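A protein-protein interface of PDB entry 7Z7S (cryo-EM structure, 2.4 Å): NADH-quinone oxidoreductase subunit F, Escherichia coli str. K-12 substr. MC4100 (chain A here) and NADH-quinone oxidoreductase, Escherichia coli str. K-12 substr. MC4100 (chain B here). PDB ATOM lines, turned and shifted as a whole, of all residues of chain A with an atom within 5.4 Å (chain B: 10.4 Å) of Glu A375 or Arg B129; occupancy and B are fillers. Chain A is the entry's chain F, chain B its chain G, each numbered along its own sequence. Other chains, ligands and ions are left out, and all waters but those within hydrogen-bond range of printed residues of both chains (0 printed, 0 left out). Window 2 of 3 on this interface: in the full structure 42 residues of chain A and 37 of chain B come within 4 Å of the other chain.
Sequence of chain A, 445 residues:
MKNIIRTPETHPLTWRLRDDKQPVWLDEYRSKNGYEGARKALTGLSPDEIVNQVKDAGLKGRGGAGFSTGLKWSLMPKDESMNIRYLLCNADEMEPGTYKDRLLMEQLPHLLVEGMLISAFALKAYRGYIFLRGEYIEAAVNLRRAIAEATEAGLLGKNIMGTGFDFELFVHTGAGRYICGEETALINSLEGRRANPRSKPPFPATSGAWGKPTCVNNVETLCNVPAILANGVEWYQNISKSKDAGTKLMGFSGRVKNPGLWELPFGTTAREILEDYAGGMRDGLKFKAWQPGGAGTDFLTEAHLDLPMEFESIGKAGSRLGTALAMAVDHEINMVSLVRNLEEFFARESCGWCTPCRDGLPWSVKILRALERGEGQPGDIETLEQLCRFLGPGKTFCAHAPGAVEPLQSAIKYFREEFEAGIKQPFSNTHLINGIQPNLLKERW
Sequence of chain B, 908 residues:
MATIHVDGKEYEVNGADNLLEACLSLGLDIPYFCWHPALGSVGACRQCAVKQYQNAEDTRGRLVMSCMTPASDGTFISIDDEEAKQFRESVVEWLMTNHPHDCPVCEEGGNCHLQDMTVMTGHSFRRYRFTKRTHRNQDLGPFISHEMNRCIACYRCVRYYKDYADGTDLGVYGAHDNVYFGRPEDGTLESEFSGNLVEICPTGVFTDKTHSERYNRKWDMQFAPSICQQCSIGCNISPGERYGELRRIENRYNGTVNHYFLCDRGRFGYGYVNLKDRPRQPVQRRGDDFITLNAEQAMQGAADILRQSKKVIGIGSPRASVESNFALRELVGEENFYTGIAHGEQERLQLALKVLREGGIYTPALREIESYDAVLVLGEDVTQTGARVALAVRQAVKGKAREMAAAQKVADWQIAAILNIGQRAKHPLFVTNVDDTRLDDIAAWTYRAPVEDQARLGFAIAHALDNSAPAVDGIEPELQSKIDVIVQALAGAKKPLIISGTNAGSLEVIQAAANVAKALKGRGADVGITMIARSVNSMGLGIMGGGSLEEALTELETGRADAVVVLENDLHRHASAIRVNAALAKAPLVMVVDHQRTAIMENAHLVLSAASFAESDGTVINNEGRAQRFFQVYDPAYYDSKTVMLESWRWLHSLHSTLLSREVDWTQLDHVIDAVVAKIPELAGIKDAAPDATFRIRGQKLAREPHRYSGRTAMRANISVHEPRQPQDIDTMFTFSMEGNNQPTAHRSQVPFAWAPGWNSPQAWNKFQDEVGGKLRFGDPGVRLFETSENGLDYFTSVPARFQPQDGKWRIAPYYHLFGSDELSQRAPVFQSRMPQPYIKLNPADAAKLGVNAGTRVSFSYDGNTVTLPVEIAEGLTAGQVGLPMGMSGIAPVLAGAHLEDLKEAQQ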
ATOM      1  N   TRP A 363       2.108  21.320 -19.869  1.00  0.00           N
ATOM      2  CA  TRP A 363       1.100  22.047 -19.103  1.00  0.00           C
ATOM      3  C   TRP A 363       0.925  23.461 -19.639  1.00  0.00           C
ATOM      4  O   TRP A 363      -0.206  23.930 -19.812  1.00  0.00           O
ATOM      5  CB  TRP A 363       1.482  22.069 -17.620  1.00  0.00           C
ATOM      6  CG  TRP A 363       0.377  22.478 -16.671  1.00  0.00           C
ATOM      7  CD1 TRP A 363      -0.857  22.951 -16.997  1.00  0.00           C
ATOM      8  CD2 TRP A 363       0.419  22.436 -15.242  1.00  0.00           C
ATOM      9  NE1 TRP A 363      -1.578  23.216 -15.871  1.00  0.00           N
ATOM     10  CE2 TRP A 363      -0.820  22.905 -14.777  1.00  0.00           C
ATOM     11  CE3 TRP A 363       1.384  22.045 -14.313  1.00  0.00           C
ATOM     12  CZ2 TRP A 363      -1.120  22.997 -13.424  1.00  0.00           C
ATOM     13  CZ3 TRP A 363       1.086  22.138 -12.974  1.00  0.00           C
ATOM     14  CH2 TRP A 363      -0.156  22.609 -12.540  1.00  0.00           C
ATOM     15  N   ALA A 370      -5.951  26.503 -24.283  1.00  0.00           N
ATOM     16  CA  ALA A 370      -7.208  26.961 -23.700  1.00  0.00           C
ATOM     17  C   ALA A 370      -7.371  28.472 -23.834  1.00  0.00           C
ATOM     18  O   ALA A 370      -8.474  28.958 -24.097  1.00  0.00           O
ATOM     19  CB  ALA A 370      -7.289  26.543 -22.234  1.00  0.00           C
ATOM     20  N   LEU A 371      -6.286  29.224 -23.645  1.00  0.00           N
ATOM     21  CA  LEU A 371      -6.344  30.678 -23.770  1.00  0.00           C
ATOM     22  C   LEU A 371      -6.642  31.104 -25.201  1.00  0.00           C
ATOM     23  O   LEU A 371      -7.366  32.078 -25.426  1.00  0.00           O
ATOM     24  CB  LEU A 371      -5.032  31.302 -23.300  1.00  0.00           C
ATOM     25  CG  LEU A 371      -4.773  31.352 -21.797  1.00  0.00           C
ATOM     26  CD1 LEU A 371      -3.421  31.972 -21.523  1.00  0.00           C
ATOM     27  CD2 LEU A 371      -5.862  32.120 -21.097  1.00  0.00           C
ATOM     28  N   ARG A 373      -8.371  29.376 -27.380  1.00  0.00           N
ATOM     29  CA  ARG A 373      -9.770  29.044 -27.621  1.00  0.00           C
ATOM     30  C   ARG A 373     -10.737  29.859 -26.775  1.00  0.00           C
ATOM     31  O   ARG A 373     -11.949  29.724 -26.955  1.00  0.00           O
ATOM     32  CB  ARG A 373     -10.014  27.560 -27.354  1.00  0.00           C
ATOM     33  CG  ARG A 373      -9.740  26.655 -28.531  1.00  0.00           C
ATOM     34  CD  ARG A 373      -9.546  25.216 -28.093  1.00  0.00           C
ATOM     35  NE  ARG A 373      -9.903  25.002 -26.695  1.00  0.00           N
ATOM     36  CZ  ARG A 373      -9.209  24.251 -25.851  1.00  0.00           C
ATOM     37  NH1 ARG A 373      -8.104  23.629 -26.226  1.00  0.00           N
ATOM     38  NH2 ARG A 373      -9.636  24.120 -24.598  1.00  0.00           N
ATOM     39  N   GLY A 374     -10.246  30.686 -25.859  1.00  0.00           N
ATOM     40  CA  GLY A 374     -11.132  31.374 -24.947  1.00  0.00           C
ATOM     41  C   GLY A 374     -11.646  30.521 -23.814  1.00  0.00           C
ATOM     42  O   GLY A 374     -12.637  30.888 -23.180  1.00  0.00           O
ATOM     43  N   GLU A 375     -11.012  29.381 -23.548  1.00  0.00           N
ATOM     44  CA  GLU A 375     -11.413  28.490 -22.470  1.00  0.00           C
ATOM     45  C   GLU A 375     -10.493  28.588 -21.262  1.00  0.00           C
ATOM     46  O   GLU A 375     -10.453  27.663 -20.448  1.00  0.00           O
ATOM     47  CB  GLU A 375     -11.472  27.048 -22.972  1.00  0.00           C
ATOM     48  CG  GLU A 375     -12.151  26.892 -24.315  1.00  0.00           C
ATOM     49  CD  GLU A 375     -12.718  25.503 -24.522  1.00  0.00           C
ATOM     50  OE1 GLU A 375     -12.257  24.565 -23.841  1.00  0.00           O
ATOM     51  OE2 GLU A 375     -13.624  25.346 -25.365  1.00  0.00           O
ATOM     52  N   GLY A 376      -9.753  29.685 -21.135  1.00  0.00           N
ATOM     53  CA  GLY A 376      -8.920  29.873 -19.968  1.00  0.00           C
ATOM     54  C   GLY A 376      -9.743  30.086 -18.712  1.00  0.00           C
ATOM     55  O   GLY A 376     -10.866  30.580 -18.746  1.00  0.00           O
ATOM     56  N   GLN A 377      -9.166  29.700 -17.589  1.00  0.00           N
ATOM     57  CA  GLN A 377      -9.797  29.762 -16.282  1.00  0.00           C
ATOM     58  C   GLN A 377      -8.870  30.521 -15.350  1.00  0.00           C
ATOM     59  O   GLN A 377      -7.667  30.605 -15.611  1.00  0.00           O
ATOM     60  CB  GLN A 377     -10.079  28.348 -15.752  1.00  0.00           C
ATOM     61  CG  GLN A 377     -11.049  27.571 -16.622  1.00  0.00           C
ATOM     62  CD  GLN A 377     -11.279  26.161 -16.141  1.00  0.00           C
ATOM     63  OE1 GLN A 377     -10.790  25.767 -15.090  1.00  0.00           O
ATOM     64  NE2 GLN A 377     -12.018  25.387 -16.916  1.00  0.00           N
ATOM     65  N   ASP A 380      -4.707  30.462 -14.549  1.00  0.00           N
ATOM     66  CA  ASP A 380      -3.914  29.976 -15.675  1.00  0.00           C
ATOM     67  C   ASP A 380      -2.680  30.837 -15.908  1.00  0.00           C
ATOM     68  O   ASP A 380      -1.589  30.312 -16.154  1.00  0.00           O
ATOM     69  CB  ASP A 380      -4.767  29.927 -16.940  1.00  0.00           C
ATOM     70  CG  ASP A 380      -5.567  28.648 -17.058  1.00  0.00           C
ATOM     71  OD1 ASP A 380      -5.429  27.767 -16.186  1.00  0.00           O
ATOM     72  OD2 ASP A 380      -6.332  28.516 -18.031  1.00  0.00           O
ATOM     73  N   GLY A 422      -8.207  35.529 -22.914  1.00  0.00           N
ATOM     74  CA  GLY A 422      -8.589  34.138 -23.048  1.00  0.00           C
ATOM     75  C   GLY A 422      -9.246  33.525 -21.834  1.00  0.00           C
ATOM     76  O   GLY A 422      -9.771  32.414 -21.931  1.00  0.00           O
ATOM     77  N   LYS A 424     -12.149  33.130 -19.793  1.00  0.00           N
ATOM     78  CA  LYS A 424     -13.580  33.368 -19.881  1.00  0.00           C
ATOM     79  C   LYS A 424     -14.413  32.468 -18.985  1.00  0.00           C
ATOM     80  O   LYS A 424     -15.471  32.896 -18.525  1.00  0.00           O
ATOM     81  CB  LYS A 424     -14.061  33.197 -21.330  1.00  0.00           C
ATOM     82  CG  LYS A 424     -13.281  34.008 -22.346  1.00  0.00           C
ATOM     83  CD  LYS A 424     -13.836  35.409 -22.480  1.00  0.00           C
ATOM     84  CE  LYS A 424     -13.586  35.964 -23.870  1.00  0.00           C
ATOM     85  NZ  LYS A 424     -13.611  34.896 -24.907  1.00  0.00           N
ATOM     86  N   GLN A 425     -13.980  31.263 -18.729  1.00  0.00           N
ATOM     87  CA  GLN A 425     -14.723  30.328 -17.904  1.00  0.00           C
ATOM     88  C   GLN A 425     -14.234  30.372 -16.464  1.00  0.00           C
ATOM     89  O   GLN A 425     -13.067  30.673 -16.212  1.00  0.00           O
ATOM     90  CB  GLN A 425     -14.581  28.904 -18.442  1.00  0.00           C
ATOM     91  CG  GLN A 425     -14.672  28.791 -19.941  1.00  0.00           C
ATOM     92  CD  GLN A 425     -14.306  27.410 -20.424  1.00  0.00           C
ATOM     93  OE1 GLN A 425     -13.770  26.601 -19.672  1.00  0.00           O
ATOM     94  NE2 GLN A 425     -14.605  27.125 -21.683  1.00  0.00           N
ATOM     95  N   PHE A 427     -12.936  28.734 -12.928  1.00  0.00           N
ATOM     96  CA  PHE A 427     -12.065  27.592 -12.683  1.00  0.00           C
ATOM     97  C   PHE A 427     -12.878  26.418 -12.156  1.00  0.00           C
ATOM     98  O   PHE A 427     -13.586  26.542 -11.154  1.00  0.00           O
ATOM     99  CB  PHE A 427     -10.950  27.935 -11.703  1.00  0.00           C
ATOM    100  CG  PHE A 427     -10.077  26.757 -11.367  1.00  0.00           C
ATOM    101  CD1 PHE A 427      -9.252  26.196 -12.329  1.00  0.00           C
ATOM    102  CD2 PHE A 427     -10.103  26.192 -10.104  1.00  0.00           C
ATOM    103  CE1 PHE A 427      -8.459  25.102 -12.037  1.00  0.00           C
ATOM    104  CE2 PHE A 427      -9.311  25.100  -9.803  1.00  0.00           C
ATOM    105  CZ  PHE A 427      -8.486  24.556 -10.771  1.00  0.00           C
ATOM    106  N   SER A 428     -12.769  25.281 -12.834  1.00  0.00           N
ATOM    107  CA  SER A 428     -13.450  24.062 -12.427  1.00  0.00           C
ATOM    108  C   SER A 428     -12.527  22.892 -12.705  1.00  0.00           C
ATOM    109  O   SER A 428     -12.123  22.674 -13.850  1.00  0.00           O
ATOM    110  CB  SER A 428     -14.776  23.884 -13.165  1.00  0.00           C
ATOM    111  OG  SER A 428     -15.178  22.527 -13.149  1.00  0.00           O
ATOM    112  N   ASN A 429     -12.189  22.153 -11.655  1.00  0.00           N
ATOM    113  CA  ASN A 429     -11.348  20.977 -11.765  1.00  0.00           C
ATOM    114  C   ASN A 429     -12.074  19.692 -11.407  1.00  0.00           C
ATOM    115  O   ASN A 429     -11.573  18.610 -11.713  1.00  0.00           O
ATOM    116  CB  ASN A 429     -10.120  21.129 -10.856  1.00  0.00           C
ATOM    117  CG  ASN A 429      -8.930  20.393 -11.378  1.00  0.00           C
ATOM    118  OD1 ASN A 429      -8.973  19.844 -12.470  1.00  0.00           O
ATOM    119  ND2 ASN A 429      -7.863  20.357 -10.601  1.00  0.00           N
ATOM    120  N   GLU B  93       4.046  17.965  -8.254  1.00  0.00           N
ATOM    121  CA  GLU B  93       2.831  18.312  -8.987  1.00  0.00           C
ATOM    122  C   GLU B  93       2.961  18.013 -10.476  1.00  0.00           C
ATOM    123  O   GLU B  93       2.014  17.527 -11.100  1.00  0.00           O
ATOM    124  CB  GLU B  93       2.491  19.784  -8.771  1.00  0.00           C
ATOM    125  CG  GLU B  93       1.272  20.257  -9.529  1.00  0.00           C
ATOM    126  CD  GLU B  93       0.910  21.684  -9.215  1.00  0.00           C
ATOM    127  OE1 GLU B  93       1.826  22.514  -9.059  1.00  0.00           O
ATOM    128  OE2 GLU B  93      -0.295  21.982  -9.124  1.00  0.00           O
ATOM    129  N   MET B  96       2.500  14.462 -10.920  1.00  0.00           N
ATOM    130  CA  MET B  96       1.103  14.120 -10.690  1.00  0.00           C
ATOM    131  C   MET B  96       0.183  14.443 -11.857  1.00  0.00           C
ATOM    132  O   MET B  96      -0.947  13.951 -11.863  1.00  0.00           O
ATOM    133  CB  MET B  96       0.574  14.842  -9.448  1.00  0.00           C
ATOM    134  CG  MET B  96       1.025  14.254  -8.144  1.00  0.00           C
ATOM    135  SD  MET B  96       0.484  12.553  -8.008  1.00  0.00           S
ATOM    136  CE  MET B  96       2.054  11.734  -7.866  1.00  0.00           C
ATOM    137  N   THR B  97       0.617  15.257 -12.824  1.00  0.00           N
ATOM    138  CA  THR B  97      -0.294  15.700 -13.878  1.00  0.00           C
ATOM    139  C   THR B  97      -0.749  14.539 -14.753  1.00  0.00           C
ATOM    140  O   THR B  97      -1.893  14.518 -15.214  1.00  0.00           O
ATOM    141  CB  THR B  97       0.355  16.783 -14.742  1.00  0.00           C
ATOM    142  OG1 THR B  97       1.644  16.350 -15.175  1.00  0.00           O
ATOM    143  CG2 THR B  97       0.491  18.071 -13.968  1.00  0.00           C
ATOM    144  N   ASN B  98       0.120  13.562 -14.982  1.00  0.00           N
ATOM    145  CA  ASN B  98      -0.217  12.415 -15.806  1.00  0.00           C
ATOM    146  C   ASN B  98      -0.421  11.135 -15.013  1.00  0.00           C
ATOM    147  O   ASN B  98      -0.703  10.097 -15.614  1.00  0.00           O
ATOM    148  CB  ASN B  98       0.866  12.187 -16.859  1.00  0.00           C
ATOM    149  CG  ASN B  98       0.977  13.329 -17.832  1.00  0.00           C
ATOM    150  OD1 ASN B  98       0.040  13.628 -18.560  1.00  0.00           O
ATOM    151  ND2 ASN B  98       2.129  13.974 -17.851  1.00  0.00           N
ATOM    152  N   PHE B 125      -3.333  19.260  -3.323  1.00  0.00           N
ATOM    153  CA  PHE B 125      -4.378  19.946  -4.065  1.00  0.00           C
ATOM    154  C   PHE B 125      -4.039  19.915  -5.545  1.00  0.00           C
ATOM    155  O   PHE B 125      -2.964  20.365  -5.947  1.00  0.00           O
ATOM    156  CB  PHE B 125      -4.527  21.390  -3.585  1.00  0.00           C
ATOM    157  CG  PHE B 125      -5.810  22.039  -4.004  1.00  0.00           C
ATOM    158  CD1 PHE B 125      -5.908  22.689  -5.222  1.00  0.00           C
ATOM    159  CD2 PHE B 125      -6.913  22.014  -3.176  1.00  0.00           C
ATOM    160  CE1 PHE B 125      -7.083  23.288  -5.607  1.00  0.00           C
ATOM    161  CE2 PHE B 125      -8.092  22.618  -3.557  1.00  0.00           C
ATOM    162  CZ  PHE B 125      -8.175  23.254  -4.773  1.00  0.00           C
ATOM    163  N   ARG B 126      -4.961  19.411  -6.352  1.00  0.00           N
ATOM    164  CA  ARG B 126      -4.774  19.316  -7.792  1.00  0.00           C
ATOM    165  C   ARG B 126      -5.406  20.527  -8.459  1.00  0.00           C
ATOM    166  O   ARG B 126      -6.585  20.812  -8.241  1.00  0.00           O
ATOM    167  CB  ARG B 126      -5.390  18.030  -8.335  1.00  0.00           C
ATOM    168  CG  ARG B 126      -5.142  17.786  -9.805  1.00  0.00           C
ATOM    169  CD  ARG B 126      -5.718  16.452 -10.220  1.00  0.00           C
ATOM    170  NE  ARG B 126      -5.456  16.137 -11.617  1.00  0.00           N
ATOM    171  CZ  ARG B 126      -4.338  15.585 -12.066  1.00  0.00           C
ATOM    172  NH1 ARG B 126      -3.335  15.299 -11.257  1.00  0.00           N
ATOM    173  NH2 ARG B 126      -4.226  15.311 -13.359  1.00  0.00           N
ATOM    174  N   ARG B 127      -4.624  21.238  -9.265  1.00  0.00           N
ATOM    175  CA  ARG B 127      -5.153  22.319 -10.077  1.00  0.00           C
ATOM    176  C   ARG B 127      -5.001  22.083 -11.570  1.00  0.00           C
ATOM    177  O   ARG B 127      -5.641  22.791 -12.352  1.00  0.00           O
ATOM    178  CB  ARG B 127      -4.494  23.654  -9.702  1.00  0.00           C
ATOM    179  CG  ARG B 127      -3.008  23.687  -9.864  1.00  0.00           C
ATOM    180  CD  ARG B 127      -2.373  24.621  -8.857  1.00  0.00           C
ATOM    181  NE  ARG B 127      -0.920  24.574  -8.950  1.00  0.00           N
ATOM    182  CZ  ARG B 127      -0.169  25.542  -9.452  1.00  0.00           C
ATOM    183  NH1 ARG B 127      -0.697  26.673  -9.882  1.00  0.00           N
ATOM    184  NH2 ARG B 127       1.146  25.371  -9.523  1.00  0.00           N
ATOM    185  N   TYR B 128      -4.181  21.120 -11.982  1.00  0.00           N
ATOM    186  CA  TYR B 128      -4.148  20.680 -13.369  1.00  0.00           C
ATOM    187  C   TYR B 128      -5.498  20.092 -13.757  1.00  0.00           C
ATOM    188  O   TYR B 128      -6.057  19.264 -13.037  1.00  0.00           O
ATOM    189  CB  TYR B 128      -3.037  19.647 -13.540  1.00  0.00           C
ATOM    190  CG  TYR B 128      -2.849  19.078 -14.924  1.00  0.00           C
ATOM    191  CD1 TYR B 128      -2.065  19.728 -15.864  1.00  0.00           C
ATOM    192  CD2 TYR B 128      -3.424  17.868 -15.276  1.00  0.00           C
ATOM    193  CE1 TYR B 128      -1.874  19.196 -17.116  1.00  0.00           C
ATOM    194  CE2 TYR B 128      -3.243  17.332 -16.520  1.00  0.00           C
ATOM    195  CZ  TYR B 128      -2.469  17.995 -17.437  1.00  0.00           C
ATOM    196  OH  TYR B 128      -2.295  17.451 -18.680  1.00  0.00           O
ATOM    197  N   ARG B 129      -6.022  20.519 -14.900  1.00  0.00           N
ATOM    198  CA  ARG B 129      -7.368  20.151 -15.303  1.00  0.00           C
ATOM    199  C   ARG B 129      -7.438  19.463 -16.656  1.00  0.00           C
ATOM    200  O   ARG B 129      -8.540  19.166 -17.123  1.00  0.00           O
ATOM    201  CB  ARG B 129      -8.268  21.391 -15.320  1.00  0.00           C
ATOM    202  CG  ARG B 129      -8.027  22.314 -16.488  1.00  0.00           C
ATOM    203  CD  ARG B 129      -9.089  23.380 -16.551  1.00  0.00           C
ATOM    204  NE  ARG B 129      -8.838  24.355 -17.603  1.00  0.00           N
ATOM    205  CZ  ARG B 129      -8.009  25.383 -17.491  1.00  0.00           C
ATOM    206  NH1 ARG B 129      -7.308  25.587 -16.391  1.00  0.00           N
ATOM    207  NH2 ARG B 129      -7.885  26.228 -18.506  1.00  0.00           N
ATOM    208  N   PHE B 130      -6.311  19.193 -17.289  1.00  0.00           N
ATOM    209  CA  PHE B 130      -6.288  18.677 -18.642  1.00  0.00           C
ATOM    210  C   PHE B 130      -6.134  17.156 -18.635  1.00  0.00           C
ATOM    211  O   PHE B 130      -6.277  16.498 -17.604  1.00  0.00           O
ATOM    212  CB  PHE B 130      -5.185  19.384 -19.420  1.00  0.00           C
ATOM    213  CG  PHE B 130      -5.256  20.879 -19.338  1.00  0.00           C
ATOM    214  CD1 PHE B 130      -6.176  21.584 -20.094  1.00  0.00           C
ATOM    215  CD2 PHE B 130      -4.407  21.582 -18.503  1.00  0.00           C
ATOM    216  CE1 PHE B 130      -6.244  22.957 -20.022  1.00  0.00           C
ATOM    217  CE2 PHE B 130      -4.473  22.959 -18.426  1.00  0.00           C
ATOM    218  CZ  PHE B 130      -5.390  23.644 -19.188  1.00  0.00           C
ATOM    219  N   THR B 131      -5.866  16.585 -19.804  1.00  0.00           N
ATOM    220  CA  THR B 131      -5.811  15.140 -19.945  1.00  0.00           C
ATOM    221  C   THR B 131      -4.495  14.581 -19.412  1.00  0.00           C
ATOM    222  O   THR B 131      -3.477  15.268 -19.335  1.00  0.00           O
ATOM    223  CB  THR B 131      -5.988  14.731 -21.407  1.00  0.00           C
ATOM    224  OG1 THR B 131      -5.040  15.429 -22.220  1.00  0.00           O
ATOM    225  CG2 THR B 131      -7.388  15.052 -21.882  1.00  0.00           C
ATOM    226  N   LYS B 132      -4.535  13.308 -19.038  1.00  0.00           N
ATOM    227  CA  LYS B 132      -3.358  12.572 -18.610  1.00  0.00           C
ATOM    228  C   LYS B 132      -2.946  11.629 -19.728  1.00  0.00           C
ATOM    229  O   LYS B 132      -3.797  10.967 -20.326  1.00  0.00           O
ATOM    230  CB  LYS B 132      -3.631  11.790 -17.323  1.00  0.00           C
ATOM    231  CG  LYS B 132      -4.464  12.553 -16.315  1.00  0.00           C
ATOM    232  CD  LYS B 132      -4.294  12.011 -14.915  1.00  0.00           C
ATOM    233  CE  LYS B 132      -5.255  10.888 -14.629  1.00  0.00           C
ATOM    234  NZ  LYS B 132      -5.539  10.783 -13.176  1.00  0.00           N
ATOM    235  N   ARG B 133      -1.650  11.590 -20.022  1.00  0.00           N
ATOM    236  CA  ARG B 133      -1.149  10.665 -21.025  1.00  0.00           C
ATOM    237  C   ARG B 133      -1.280   9.230 -20.533  1.00  0.00           C
ATOM    238  O   ARG B 133      -1.281   8.959 -19.333  1.00  0.00           O
ATOM    239  CB  ARG B 133       0.306  10.971 -21.368  1.00  0.00           C
ATOM    240  CG  ARG B 133       1.290  10.775 -20.232  1.00  0.00           C
ATOM    241  CD  ARG B 133       2.121   9.519 -20.405  1.00  0.00           C
ATOM    242  NE  ARG B 133       2.912   9.205 -19.219  1.00  0.00           N
ATOM    243  CZ  ARG B 133       2.450   8.579 -18.144  1.00  0.00           C
ATOM    244  NH1 ARG B 133       1.188   8.200 -18.051  1.00  0.00           N
ATOM    245  NH2 ARG B 133       3.279   8.330 -17.137  1.00  0.00           N
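The guanidinium group of Arg B129 lies close to the side-chain amide nitrogen of Gln A377, at 3.4 Å. The guanidinium group (NH2) of Arg B129 lies within salt-bridge range of the side-chain carboxylate (OD2) of Asp A380, 2.8 Å away. The side-chain amide nitrogen (ND2) of Asn A429 lies within hydrogen-bond range of the backbone carbonyl oxygen (O) of Arg B126 (2.7 Å). OD1 of Asn A429 sits close to O of Tyr B128, 3.0 Å away.
O of Ala A370 is in hydrogen-bond range of N of Glu A375. OD2 of Asp A380 lies within hydrogen-bond range of N of Gln A377 (3.1 Å). NE2 of Gln A377 sits at hydrogen-bond distance from OE1 of Gln A425, at 3.5 Å. OE1 of Gln A377 sits at hydrogen-bond distance from N of Ser A428, 3.0 Å away. The side-chain carboxylate of Glu B93 is in salt-bridge range of the guanidinium group of Arg B127. O of Met B96 is in hydrogen-bond range of NH1 of Arg B126.
Glu B93 touches Trp A363 (OE2 to CH2, 3.5 Å). Trp A363 touches Tyr B128. NE1 of Trp A363 touches CE2 of Phe B130, 3.9 Å away. CB of Ala A370 touches NH2 of Arg B129 (3.8 Å). Glu A375 touches Arg B129. Phe A427 touches Arg B127. ND2 of Asn A429 touches CA of Arg B127 (3.4 Å). Asn A429 touches Arg B129 (OD1 to CA, 3.3 Å).
Of the printed residues of chain B, Trp A363 touches Glu B93, Tyr B128 and Phe B130. Ala A370 touches just one residue of chain B: Arg B129. Leu A371 touches none of the printed residues of chain B. No residue of chain B comes within 4 Å of Gly A374. Of chain B, only Arg B129 (3.5 Å) comes within 4 Å of Glu A375. Of the printed residues of chain B, Asp A380 touches Arg B129. No residue of chain B comes within 4 Å of Gln A425. Of the printed residues of chain A, Arg B126 touches Asn A429. Of the printed residues of chain A, Arg B127 touches Phe A427 and Asn A429. Of chain A, only Ala A370, Glu A375, Gln A377, Asp A380 and Asn A429 come within 4 Å of Arg B129. The nearest printed residue of chain B that does not touch Trp A363 is Arg B127 (4.1 Å).
Of the 13 printed residues of chain B, 6 touch a printed residue of chain A. Printed residues of chain B that touch a printed residue of chain A: Glu B93, Arg B126, Arg B127, Tyr B128, Arg B129 and Phe B130. Of the 15 printed residues of chain A, 7 touch a printed residue of chain B. Hydrophobic or aromatic side chains of chain A that line the printed part of chain B: Trp A363, Ala A370 and Phe A427. Among the printed residues, 12 pairs touch across the chains. Among the printed residues, Asp or Glu carboxylates within 4 Å of a Lys or Arg side-chain nitrogen of the other chain: Asp A380 with Arg B129 (2.8 Å).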
